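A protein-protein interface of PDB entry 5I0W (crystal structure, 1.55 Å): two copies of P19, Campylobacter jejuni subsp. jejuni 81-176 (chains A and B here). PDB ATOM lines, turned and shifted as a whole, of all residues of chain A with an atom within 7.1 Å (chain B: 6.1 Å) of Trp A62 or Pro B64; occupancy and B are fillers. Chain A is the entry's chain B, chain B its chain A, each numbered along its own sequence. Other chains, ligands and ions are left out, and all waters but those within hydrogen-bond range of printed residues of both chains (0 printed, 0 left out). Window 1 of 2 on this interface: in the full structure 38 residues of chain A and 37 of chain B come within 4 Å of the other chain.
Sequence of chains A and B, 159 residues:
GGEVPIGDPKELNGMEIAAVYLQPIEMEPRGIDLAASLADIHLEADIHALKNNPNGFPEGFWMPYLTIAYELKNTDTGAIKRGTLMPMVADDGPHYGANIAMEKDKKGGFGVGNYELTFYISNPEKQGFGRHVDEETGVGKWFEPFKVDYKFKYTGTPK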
ATOM      1  N   ALA A  45      26.884  -0.582  21.153  1.00  0.00           N
ATOM      2  CA  ALA A  45      26.711  -1.099  19.782  1.00  0.00           C
ATOM      3  C   ALA A  45      27.628  -0.270  18.906  1.00  0.00           C
ATOM      4  O   ALA A  45      27.528   0.981  18.891  1.00  0.00           O
ATOM      5  CB  ALA A  45      25.265  -0.984  19.337  1.00  0.00           C
ATOM      6  N   ASP A  46      28.544  -0.951  18.205  1.00  0.00           N
ATOM      7  CA  ASP A  46      29.473  -0.317  17.268  1.00  0.00           C
ATOM      8  C   ASP A  46      28.956  -0.566  15.860  1.00  0.00           C
ATOM      9  O   ASP A  46      28.994  -1.698  15.381  1.00  0.00           O
ATOM     10  CB  ASP A  46      30.882  -0.902  17.380  1.00  0.00           C
ATOM     11  CG  ASP A  46      31.763  -0.186  18.375  1.00  0.00           C
ATOM     12  OD1 ASP A  46      31.646   1.035  18.571  1.00  0.00           O
ATOM     13  OD2 ASP A  46      32.611  -0.863  18.962  1.00  0.00           O
ATOM     14  N   ILE A  47      28.477   0.481  15.198  1.00  0.00           N
ATOM     15  CA  ILE A  47      27.763   0.357  13.909  1.00  0.00           C
ATOM     16  C   ILE A  47      28.334   1.347  12.902  1.00  0.00           C
ATOM     17  O   ILE A  47      28.248   2.571  13.101  1.00  0.00           O
ATOM     18  CB  ILE A  47      26.260   0.626  14.087  1.00  0.00           C
ATOM     19  CG1 ILE A  47      25.718  -0.261  15.213  1.00  0.00           C
ATOM     20  CG2 ILE A  47      25.477   0.375  12.795  1.00  0.00           C
ATOM     21  CD1 ILE A  47      24.220  -0.118  15.443  1.00  0.00           C
ATOM     22  N   HIS A  48      28.953   0.810  11.843  1.00  0.00           N
ATOM     23  CA  HIS A  48      29.629   1.648  10.837  1.00  0.00           C
ATOM     24  C   HIS A  48      29.314   1.165   9.475  1.00  0.00           C
ATOM     25  O   HIS A  48      28.987  -0.001   9.273  1.00  0.00           O
ATOM     26  CB  HIS A  48      31.142   1.641  11.051  1.00  0.00           C
ATOM     27  CG  HIS A  48      31.530   2.189  12.398  1.00  0.00           C
ATOM     28  ND1 HIS A  48      31.578   1.411  13.521  1.00  0.00           N
ATOM     29  CD2 HIS A  48      31.774   3.498  12.811  1.00  0.00           C
ATOM     30  CE1 HIS A  48      31.892   2.192  14.572  1.00  0.00           C
ATOM     31  NE2 HIS A  48      32.000   3.462  14.141  1.00  0.00           N
ATOM     32  N   ALA A  49      29.391   2.066   8.510  1.00  0.00           N
ATOM     33  CA  ALA A  49      29.119   1.706   7.122  1.00  0.00           C
ATOM     34  C   ALA A  49      30.160   0.767   6.542  1.00  0.00           C
ATOM     35  O   ALA A  49      31.346   0.931   6.795  1.00  0.00           O
ATOM     36  CB  ALA A  49      29.045   2.972   6.280  1.00  0.00           C
ATOM     37  N   PHE A  57      26.228   6.199   2.900  1.00  0.00           N
ATOM     38  CA  PHE A  57      27.215   6.479   3.955  1.00  0.00           C
ATOM     39  C   PHE A  57      28.614   6.040   3.575  1.00  0.00           C
ATOM     40  O   PHE A  57      28.816   4.900   3.195  1.00  0.00           O
ATOM     41  CB  PHE A  57      26.814   5.862   5.297  1.00  0.00           C
ATOM     42  CG  PHE A  57      25.787   6.677   6.017  1.00  0.00           C
ATOM     43  CD1 PHE A  57      24.434   6.577   5.693  1.00  0.00           C
ATOM     44  CD2 PHE A  57      26.198   7.625   6.951  1.00  0.00           C
ATOM     45  CE1 PHE A  57      23.488   7.382   6.352  1.00  0.00           C
ATOM     46  CE2 PHE A  57      25.270   8.415   7.602  1.00  0.00           C
ATOM     47  CZ  PHE A  57      23.932   8.306   7.291  1.00  0.00           C
ATOM     48  N   PRO A  58      29.589   6.954   3.676  1.00  0.00           N
ATOM     49  CA  PRO A  58      30.967   6.560   3.384  1.00  0.00           C
ATOM     50  C   PRO A  58      31.437   5.414   4.266  1.00  0.00           C
ATOM     51  O   PRO A  58      31.096   5.352   5.444  1.00  0.00           O
ATOM     52  CB  PRO A  58      31.769   7.809   3.785  1.00  0.00           C
ATOM     53  CG  PRO A  58      30.813   8.915   3.477  1.00  0.00           C
ATOM     54  CD  PRO A  58      29.472   8.405   3.925  1.00  0.00           C
ATOM     55  N   GLU A  59      32.208   4.514   3.677  1.00  0.00           N
ATOM     56  CA  GLU A  59      32.804   3.392   4.399  1.00  0.00           C
ATOM     57  C   GLU A  59      33.433   3.863   5.675  1.00  0.00           C
ATOM     58  O   GLU A  59      34.206   4.827   5.681  1.00  0.00           O
ATOM     59  CB  GLU A  59      33.863   2.683   3.529  1.00  0.00           C
ATOM     60  CG  GLU A  59      34.381   1.408   4.172  1.00  0.00           C
ATOM     61  CD  GLU A  59      35.622   0.835   3.503  1.00  0.00           C
ATOM     62  OE1 GLU A  59      36.202   1.485   2.603  1.00  0.00           O
ATOM     63  OE2 GLU A  59      36.036  -0.269   3.917  1.00  0.00           O
ATOM     64  N   GLY A  60      33.081   3.188   6.769  1.00  0.00           N
ATOM     65  CA  GLY A  60      33.663   3.503   8.077  1.00  0.00           C
ATOM     66  C   GLY A  60      32.934   4.574   8.873  1.00  0.00           C
ATOM     67  O   GLY A  60      33.134   4.683  10.083  1.00  0.00           O
ATOM     68  N   PHE A  61      32.085   5.365   8.214  1.00  0.00           N
ATOM     69  CA  PHE A  61      31.280   6.344   8.944  1.00  0.00           C
ATOM     70  C   PHE A  61      30.392   5.678   9.985  1.00  0.00           C
ATOM     71  O   PHE A  61      29.838   4.600   9.764  1.00  0.00           O
ATOM     72  CB  PHE A  61      30.418   7.196   7.994  1.00  0.00           C
ATOM     73  CG  PHE A  61      31.071   8.498   7.561  1.00  0.00           C
ATOM     74  CD1 PHE A  61      32.458   8.626   7.465  1.00  0.00           C
ATOM     75  CD2 PHE A  61      30.278   9.567   7.187  1.00  0.00           C
ATOM     76  CE1 PHE A  61      33.051   9.830   7.052  1.00  0.00           C
ATOM     77  CE2 PHE A  61      30.859  10.769   6.764  1.00  0.00           C
ATOM     78  CZ  PHE A  61      32.244  10.889   6.684  1.00  0.00           C
ATOM     79  N   TRP A  62      30.242   6.343  11.121  1.00  0.00           N
ATOM     80  CA  TRP A  62      29.240   5.936  12.089  1.00  0.00           C
ATOM     81  C   TRP A  62      27.860   6.055  11.502  1.00  0.00           C
ATOM     82  O   TRP A  62      27.586   7.002  10.785  1.00  0.00           O
ATOM     83  CB  TRP A  62      29.383   6.809  13.331  1.00  0.00           C
ATOM     84  CG  TRP A  62      28.404   6.455  14.423  1.00  0.00           C
ATOM     85  CD1 TRP A  62      28.262   5.231  15.089  1.00  0.00           C
ATOM     86  CD2 TRP A  62      27.427   7.342  15.041  1.00  0.00           C
ATOM     87  NE1 TRP A  62      27.260   5.300  16.023  1.00  0.00           N
ATOM     88  CE2 TRP A  62      26.737   6.549  16.066  1.00  0.00           C
ATOM     89  CE3 TRP A  62      27.077   8.687  14.860  1.00  0.00           C
ATOM     90  CZ2 TRP A  62      25.729   7.089  16.862  1.00  0.00           C
ATOM     91  CZ3 TRP A  62      26.057   9.224  15.662  1.00  0.00           C
ATOM     92  CH2 TRP A  62      25.391   8.435  16.631  1.00  0.00           C
ATOM     93  N   MET A  63      26.982   5.087  11.768  1.00  0.00           N
ATOM     94  CA  MET A  63      25.583   5.167  11.309  1.00  0.00           C
ATOM     95  C   MET A  63      24.713   5.886  12.344  1.00  0.00           C
ATOM     96  O   MET A  63      24.490   5.347  13.428  1.00  0.00           O
ATOM     97  CB  MET A  63      25.020   3.757  11.032  1.00  0.00           C
ATOM     98  CG  MET A  63      25.839   2.933  10.055  1.00  0.00           C
ATOM     99  SD  MET A  63      25.840   3.654   8.401  1.00  0.00           S
ATOM    100  CE  MET A  63      24.118   3.575   7.950  1.00  0.00           C
ATOM    101  N   PRO A  64      24.268   7.113  12.045  1.00  0.00           N
ATOM    102  CA  PRO A  64      23.579   7.970  13.023  1.00  0.00           C
ATOM    103  C   PRO A  64      22.060   7.848  12.940  1.00  0.00           C
ATOM    104  O   PRO A  64      21.522   7.325  11.962  1.00  0.00           O
ATOM    105  CB  PRO A  64      24.009   9.372  12.581  1.00  0.00           C
ATOM    106  CG  PRO A  64      23.961   9.240  11.075  1.00  0.00           C
ATOM    107  CD  PRO A  64      24.392   7.815  10.748  1.00  0.00           C
ATOM    108  N   TYR A  65      21.373   8.314  13.983  1.00  0.00           N
ATOM    109  CA  TYR A  65      19.900   8.406  14.033  1.00  0.00           C
ATOM    110  C   TYR A  65      19.183   7.074  13.999  1.00  0.00           C
ATOM    111  O   TYR A  65      18.001   7.017  13.676  1.00  0.00           O
ATOM    112  CB  TYR A  65      19.357   9.320  12.916  1.00  0.00           C
ATOM    113  CG  TYR A  65      19.847  10.741  12.993  1.00  0.00           C
ATOM    114  CD1 TYR A  65      19.154  11.699  13.734  1.00  0.00           C
ATOM    115  CD2 TYR A  65      20.992  11.125  12.312  1.00  0.00           C
ATOM    116  CE1 TYR A  65      19.607  13.015  13.782  1.00  0.00           C
ATOM    117  CE2 TYR A  65      21.470  12.421  12.367  1.00  0.00           C
ATOM    118  CZ  TYR A  65      20.770  13.356  13.099  1.00  0.00           C
ATOM    119  OH  TYR A  65      21.228  14.665  13.134  1.00  0.00           O
ATOM    120  N   LEU A  66      19.893   6.003  14.369  1.00  0.00           N
ATOM    121  CA  LEU A  66      19.234   4.704  14.489  1.00  0.00           C
ATOM    122  C   LEU A  66      18.456   4.660  15.792  1.00  0.00           C
ATOM    123  O   LEU A  66      18.876   5.286  16.783  1.00  0.00           O
ATOM    124  CB  LEU A  66      20.250   3.559  14.475  1.00  0.00           C
ATOM    125  CG  LEU A  66      21.070   3.414  13.185  1.00  0.00           C
ATOM    126  CD1 LEU A  66      22.113   2.313  13.297  1.00  0.00           C
ATOM    127  CD2 LEU A  66      20.153   3.139  11.983  1.00  0.00           C
ATOM    128  N   MET A  86      21.588   4.590  23.723  1.00  0.00           N
ATOM    129  CA  MET A  86      21.534   6.021  23.452  1.00  0.00           C
ATOM    130  C   MET A  86      22.728   6.475  22.619  1.00  0.00           C
ATOM    131  O   MET A  86      23.837   5.987  22.812  1.00  0.00           O
ATOM    132  CB  MET A  86      21.545   6.775  24.783  1.00  0.00           C
ATOM    133  CG  MET A  86      20.246   6.641  25.547  1.00  0.00           C
ATOM    134  SD  MET A  86      20.458   6.730  27.329  1.00  0.00           S
ATOM    135  CE  MET A  86      21.339   5.202  27.643  1.00  0.00           C
ATOM    136  N   PRO A  87      22.514   7.421  21.689  1.00  0.00           N
ATOM    137  CA  PRO A  87      23.660   7.920  20.919  1.00  0.00           C
ATOM    138  C   PRO A  87      24.492   8.860  21.754  1.00  0.00           C
ATOM    139  O   PRO A  87      23.947   9.691  22.471  1.00  0.00           O
ATOM    140  CB  PRO A  87      23.015   8.703  19.765  1.00  0.00           C
ATOM    141  CG  PRO A  87      21.702   9.139  20.338  1.00  0.00           C
ATOM    142  CD  PRO A  87      21.247   8.029  21.251  1.00  0.00           C
ATOM    143  N   MET A  88      25.799   8.680  21.691  1.00  0.00           N
ATOM    144  CA  MET A  88      26.725   9.504  22.474  1.00  0.00           C
ATOM    145  C   MET A  88      28.126   9.385  21.920  1.00  0.00           C
ATOM    146  O   MET A  88      28.379   8.574  21.040  1.00  0.00           O
ATOM    147  CB  MET A  88      26.690   9.063  23.927  1.00  0.00           C
ATOM    148  CG  MET A  88      27.253   7.669  24.104  1.00  0.00           C
ATOM    149  SD  MET A  88      27.050   7.044  25.778  1.00  0.00           S
ATOM    150  CE  MET A  88      25.377   6.463  25.821  1.00  0.00           C
ATOM    151  N   VAL A  89      29.038  10.214  22.432  1.00  0.00           N
ATOM    152  CA  VAL A  89      30.422  10.164  21.979  1.00  0.00           C
ATOM    153  C   VAL A  89      31.352   9.919  23.170  1.00  0.00           C
ATOM    154  O   VAL A  89      31.136  10.456  24.256  1.00  0.00           O
ATOM    155  CB  VAL A  89      30.798  11.458  21.195  1.00  0.00           C
ATOM    156  CG1 VAL A  89      30.770  12.713  22.066  1.00  0.00           C
ATOM    157  CG2 VAL A  89      32.118  11.300  20.465  1.00  0.00           C
ATOM    158  N   GLY A  93      35.103   7.963  19.823  1.00  0.00           N
ATOM    159  CA  GLY A  93      34.120   8.374  18.808  1.00  0.00           C
ATOM    160  C   GLY A  93      32.693   8.058  19.176  1.00  0.00           C
ATOM    161  O   GLY A  93      32.419   7.575  20.285  1.00  0.00           O
ATOM    162  N   PRO A  94      31.757   8.313  18.246  1.00  0.00           N
ATOM    163  CA  PRO A  94      30.352   8.096  18.568  1.00  0.00           C
ATOM    164  C   PRO A  94      29.980   6.613  18.581  1.00  0.00           C
ATOM    165  O   PRO A  94      30.616   5.805  17.886  1.00  0.00           O
ATOM    166  CB  PRO A  94      29.615   8.841  17.452  1.00  0.00           C
ATOM    167  CG  PRO A  94      30.585   8.800  16.294  1.00  0.00           C
ATOM    168  CD  PRO A  94      31.933   8.969  16.936  1.00  0.00           C
ATOM    169  N   HIS A  95      28.979   6.302  19.394  1.00  0.00           N
ATOM    170  CA  HIS A  95      28.383   4.961  19.438  1.00  0.00           C
ATOM    171  C   HIS A  95      27.015   5.031  20.032  1.00  0.00           C
ATOM    172  O   HIS A  95      26.510   6.115  20.387  1.00  0.00           O
ATOM    173  CB  HIS A  95      29.269   4.010  20.279  1.00  0.00           C
ATOM    174  CG  HIS A  95      29.454   4.448  21.722  1.00  0.00           C
ATOM    175  ND1 HIS A  95      30.577   5.058  22.146  1.00  0.00           N
ATOM    176  CD2 HIS A  95      28.600   4.375  22.830  1.00  0.00           C
ATOM    177  CE1 HIS A  95      30.453   5.353  23.460  1.00  0.00           C
ATOM    178  NE2 HIS A  95      29.245   4.946  23.874  1.00  0.00           N
ATOM    179  N   TYR A  96      26.389   3.867  20.152  1.00  0.00           N
ATOM    180  CA  TYR A  96      25.137   3.757  20.911  1.00  0.00           C
ATOM    181  C   TYR A  96      25.460   2.934  22.146  1.00  0.00           C
ATOM    182  O   TYR A  96      26.093   1.881  22.052  1.00  0.00           O
ATOM    183  CB  TYR A  96      24.058   3.051  20.068  1.00  0.00           C
ATOM    184  CG  TYR A  96      23.695   3.770  18.797  1.00  0.00           C
ATOM    185  CD1 TYR A  96      22.702   4.746  18.781  1.00  0.00           C
ATOM    186  CD2 TYR A  96      24.358   3.459  17.599  1.00  0.00           C
ATOM    187  CE1 TYR A  96      22.368   5.413  17.599  1.00  0.00           C
ATOM    188  CE2 TYR A  96      24.033   4.112  16.411  1.00  0.00           C
ATOM    189  CZ  TYR A  96      23.060   5.086  16.424  1.00  0.00           C
ATOM    190  OH  TYR A  96      22.729   5.754  15.262  1.00  0.00           O
ATOM    191  N   PHE B  57      35.388  13.186  18.084  1.00  0.00           N
ATOM    192  CA  PHE B  57      35.092  12.789  16.706  1.00  0.00           C
ATOM    193  C   PHE B  57      36.343  12.605  15.865  1.00  0.00           C
ATOM    194  O   PHE B  57      37.191  13.474  15.834  1.00  0.00           O
ATOM    195  CB  PHE B  57      34.114  13.748  16.027  1.00  0.00           C
ATOM    196  CG  PHE B  57      32.713  13.525  16.460  1.00  0.00           C
ATOM    197  CD1 PHE B  57      32.256  14.014  17.680  1.00  0.00           C
ATOM    198  CD2 PHE B  57      31.867  12.748  15.670  1.00  0.00           C
ATOM    199  CE1 PHE B  57      30.946  13.771  18.081  1.00  0.00           C
ATOM    200  CE2 PHE B  57      30.574  12.490  16.077  1.00  0.00           C
ATOM    201  CZ  PHE B  57      30.116  12.997  17.275  1.00  0.00           C
ATOM    202  N   PHE B  61      34.916  12.723  10.142  1.00  0.00           N
ATOM    203  CA  PHE B  61      33.552  12.232  10.438  1.00  0.00           C
ATOM    204  C   PHE B  61      32.555  13.373  10.321  1.00  0.00           C
ATOM    205  O   PHE B  61      32.831  14.508  10.711  1.00  0.00           O
ATOM    206  CB  PHE B  61      33.438  11.663  11.866  1.00  0.00           C
ATOM    207  CG  PHE B  61      33.524  10.159  11.961  1.00  0.00           C
ATOM    208  CD1 PHE B  61      34.187   9.392  11.003  1.00  0.00           C
ATOM    209  CD2 PHE B  61      32.952   9.510  13.039  1.00  0.00           C
ATOM    210  CE1 PHE B  61      34.248   8.003  11.123  1.00  0.00           C
ATOM    211  CE2 PHE B  61      33.040   8.126  13.177  1.00  0.00           C
ATOM    212  CZ  PHE B  61      33.685   7.379  12.214  1.00  0.00           C
ATOM    213  N   TRP B  62      31.397  13.060   9.775  1.00  0.00           N
ATOM    214  CA  TRP B  62      30.271  13.980   9.830  1.00  0.00           C
ATOM    215  C   TRP B  62      29.885  14.310  11.264  1.00  0.00           C
ATOM    216  O   TRP B  62      29.860  13.426  12.129  1.00  0.00           O
ATOM    217  CB  TRP B  62      29.104  13.347   9.082  1.00  0.00           C
ATOM    218  CG  TRP B  62      27.904  14.259   8.997  1.00  0.00           C
ATOM    219  CD1 TRP B  62      27.833  15.542   8.441  1.00  0.00           C
ATOM    220  CD2 TRP B  62      26.559  13.969   9.472  1.00  0.00           C
ATOM    221  NE1 TRP B  62      26.560  16.044   8.553  1.00  0.00           N
ATOM    222  CE2 TRP B  62      25.745  15.141   9.159  1.00  0.00           C
ATOM    223  CE3 TRP B  62      25.962  12.883  10.084  1.00  0.00           C
ATOM    224  CZ2 TRP B  62      24.388  15.203   9.465  1.00  0.00           C
ATOM    225  CZ3 TRP B  62      24.607  12.962  10.411  1.00  0.00           C
ATOM    226  CH2 TRP B  62      23.839  14.097  10.101  1.00  0.00           C
ATOM    227  N   MET B  63      29.643  15.600  11.551  1.00  0.00           N
ATOM    228  CA  MET B  63      29.168  15.983  12.881  1.00  0.00           C
ATOM    229  C   MET B  63      27.643  15.872  12.971  1.00  0.00           C
ATOM    230  O   MET B  63      26.946  16.652  12.332  1.00  0.00           O
ATOM    231  CB  MET B  63      29.621  17.411  13.248  1.00  0.00           C
ATOM    232  CG  MET B  63      31.108  17.635  13.152  1.00  0.00           C
ATOM    233  SD  MET B  63      32.018  16.691  14.382  1.00  0.00           S
ATOM    234  CE  MET B  63      31.466  17.418  15.914  1.00  0.00           C
ATOM    235  N   PRO B  64      27.126  14.870  13.698  1.00  0.00           N
ATOM    236  CA  PRO B  64      25.705  14.559  13.755  1.00  0.00           C
ATOM    237  C   PRO B  64      24.983  15.253  14.916  1.00  0.00           C
ATOM    238  O   PRO B  64      25.620  15.732  15.882  1.00  0.00           O
ATOM    239  CB  PRO B  64      25.724  13.045  13.996  1.00  0.00           C
ATOM    240  CG  PRO B  64      26.915  12.864  14.913  1.00  0.00           C
ATOM    241  CD  PRO B  64      27.886  13.989  14.608  1.00  0.00           C
ATOM    242  N   TYR B  65      23.662  15.306  14.813  1.00  0.00           N
ATOM    243  CA  TYR B  65      22.787  15.844  15.866  1.00  0.00           C
ATOM    244  C   TYR B  65      22.988  17.335  16.165  1.00  0.00           C
ATOM    245  O   TYR B  65      22.570  17.815  17.236  1.00  0.00           O
ATOM    246  CB  TYR B  65      22.901  15.022  17.167  1.00  0.00           C
ATOM    247  CG  TYR B  65      22.511  13.564  17.029  1.00  0.00           C
ATOM    248  CD1 TYR B  65      23.447  12.616  16.604  1.00  0.00           C
ATOM    249  CD2 TYR B  65      21.221  13.134  17.322  1.00  0.00           C
ATOM    250  CE1 TYR B  65      23.100  11.286  16.462  1.00  0.00           C
ATOM    251  CE2 TYR B  65      20.880  11.793  17.194  1.00  0.00           C
ATOM    252  CZ  TYR B  65      21.828  10.891  16.748  1.00  0.00           C
ATOM    253  OH  TYR B  65      21.494   9.570  16.636  1.00  0.00           O
ATOM    254  N   LEU B  66      23.563  18.053  15.205  1.00  0.00           N
ATOM    255  CA  LEU B  66      23.670  19.515  15.332  1.00  0.00           C
ATOM    256  C   LEU B  66      22.322  20.138  15.013  1.00  0.00           C
ATOM    257  O   LEU B  66      21.557  19.631  14.189  1.00  0.00           O
ATOM    258  CB  LEU B  66      24.726  20.098  14.388  1.00  0.00           C
ATOM    259  CG  LEU B  66      26.163  19.631  14.601  1.00  0.00           C
ATOM    260  CD1 LEU B  66      27.056  20.173  13.505  1.00  0.00           C
ATOM    261  CD2 LEU B  66      26.660  20.047  15.977  1.00  0.00           C
ATOM    262  N   TYR B  96      23.473  18.410   6.276  1.00  0.00           N
ATOM    263  CA  TYR B  96      22.272  19.121   6.701  1.00  0.00           C
ATOM    264  C   TYR B  96      21.815  19.935   5.511  1.00  0.00           C
ATOM    265  O   TYR B  96      22.646  20.616   4.880  1.00  0.00           O
ATOM    266  CB  TYR B  96      22.578  20.050   7.876  1.00  0.00           C
ATOM    267  CG  TYR B  96      23.089  19.325   9.095  1.00  0.00           C
ATOM    268  CD1 TYR B  96      22.194  18.831  10.044  1.00  0.00           C
ATOM    269  CD2 TYR B  96      24.463  19.145   9.298  1.00  0.00           C
ATOM    270  CE1 TYR B  96      22.650  18.142  11.157  1.00  0.00           C
ATOM    271  CE2 TYR B  96      24.934  18.454  10.403  1.00  0.00           C
ATOM    272  CZ  TYR B  96      24.026  17.983  11.339  1.00  0.00           C
ATOM    273  OH  TYR B  96      24.420  17.269  12.457  1.00  0.00           O
ATOM    274  N   PRO B 124      25.457  19.029  19.894  1.00  0.00           N
ATOM    275  CA  PRO B 124      24.540  17.883  19.881  1.00  0.00           C
ATOM    276  C   PRO B 124      23.763  17.643  21.164  1.00  0.00           C
ATOM    277  O   PRO B 124      22.729  16.977  21.142  1.00  0.00           O
ATOM    278  CB  PRO B 124      25.491  16.703  19.618  1.00  0.00           C
ATOM    279  CG  PRO B 124      26.575  17.304  18.797  1.00  0.00           C
ATOM    280  CD  PRO B 124      26.820  18.634  19.481  1.00  0.00           C
ATOM    281  N   PHE B 129      21.919  14.064  22.499  1.00  0.00           N
ATOM    282  CA  PHE B 129      23.134  13.275  22.232  1.00  0.00           C
ATOM    283  C   PHE B 129      24.118  13.427  23.394  1.00  0.00           C
ATOM    284  O   PHE B 129      24.390  14.545  23.837  1.00  0.00           O
ATOM    285  CB  PHE B 129      23.749  13.791  20.925  1.00  0.00           C
ATOM    286  CG  PHE B 129      24.958  13.020  20.450  1.00  0.00           C
ATOM    287  CD1 PHE B 129      24.808  11.924  19.628  1.00  0.00           C
ATOM    288  CD2 PHE B 129      26.239  13.394  20.833  1.00  0.00           C
ATOM    289  CE1 PHE B 129      25.923  11.224  19.165  1.00  0.00           C
ATOM    290  CE2 PHE B 129      27.351  12.696  20.390  1.00  0.00           C
ATOM    291  CZ  PHE B 129      27.192  11.604  19.542  1.00  0.00           C
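Gly A60 touches Phe B61. Trp B62 touches Phe A61. Trp A62 touches Phe B61 (N to CZ, 3.8 Å). Pro B64 touches Trp A62 (CG to CZ3, 3.8 Å). CH2 of Trp A62 touches CE1 of Tyr B65, 3.7 Å away. Trp A62 touches Phe B129. CG of Pro A64 touches CZ3 of Trp B62, 3.8 Å away. Pro A87 touches Phe B129. Met A88 touches Phe B129 (C to CZ, 3.4 Å). CG2 of Val A89 touches CE1 of Phe B57 (3.6 Å).
Of chain B, only Phe B61, Pro B64, Tyr B65 and Phe B129 come within 4 Å of Trp A62. Of chain A, only Trp A62 comes within 4 Å of Pro B64. Printed residues of chain A within 4 Å of Phe B129: Trp A62, Pro A87, Met A88 and Val A89. Of the printed residues of chain B, Pro A87 touches Tyr B65 (3.6 Å) and Phe B129 (3.7 Å). Of the printed residues of chain A, Phe B61 touches Gly A60 (3.5 Å) and Trp A62 (3.8 Å). Gly A93 touches none of the printed residues of chain B. Leu B66 touches none of the printed residues of chain A. The nearest residue of chain B that does not touch Trp A62 is Phe B57 (5.3 Å). The nearest printed residue of chain A that does not touch Tyr B65 is Pro A64 (4.1 Å).
OH of Tyr B96 lies within hydrogen-bond range of N of Tyr B65 (3.2 Å). The backbone NH (N) of Phe B129 is in hydrogen-bond range of the backbone carbonyl oxygen (O) of Pro B124 (3.3 Å). The backbone carbonyl oxygen (O) of Ala A49 lies within hydrogen-bond range of the backbone NH (N) of Gly A60 (2.8 Å). The backbone NH (N) of Ala A49 lies within hydrogen-bond range of the backbone carbonyl oxygen (O) of Phe A61. N of Tyr A65 sits at hydrogen-bond distance from OH of Tyr A96 (3.2 Å).
Phe A61 touches Trp B62, and with the chains exchanged Trp A62 touches Phe B61. Trp A62 touches Pro B64, and with the chains exchanged Pro A64 touches Trp B62. Trp A62 touches Tyr B65, and with the chains exchanged Tyr A65 touches Trp B62. Tyr A65 touches its own counterpart, Tyr B65. Of the 15 pairs that touch across the chains among the printed residues, 7 have their exchanged pair printed and touching as well.
OH of Tyr B65 is in hydrogen-bond range of N of Tyr A65 (2.9 Å).
Of the 10 printed residues of chain B, 6 touch a printed residue of chain A. Along chain B the printed residues that touch a printed residue of chain A span positions 57 to 129. Of the 23 printed residues of chain A, 9 touch a printed residue of chain B. Among the printed residues, no Asp or Glu carboxylate lies within 4 Å of a Lys or Arg side-chain nitrogen of the other chain.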
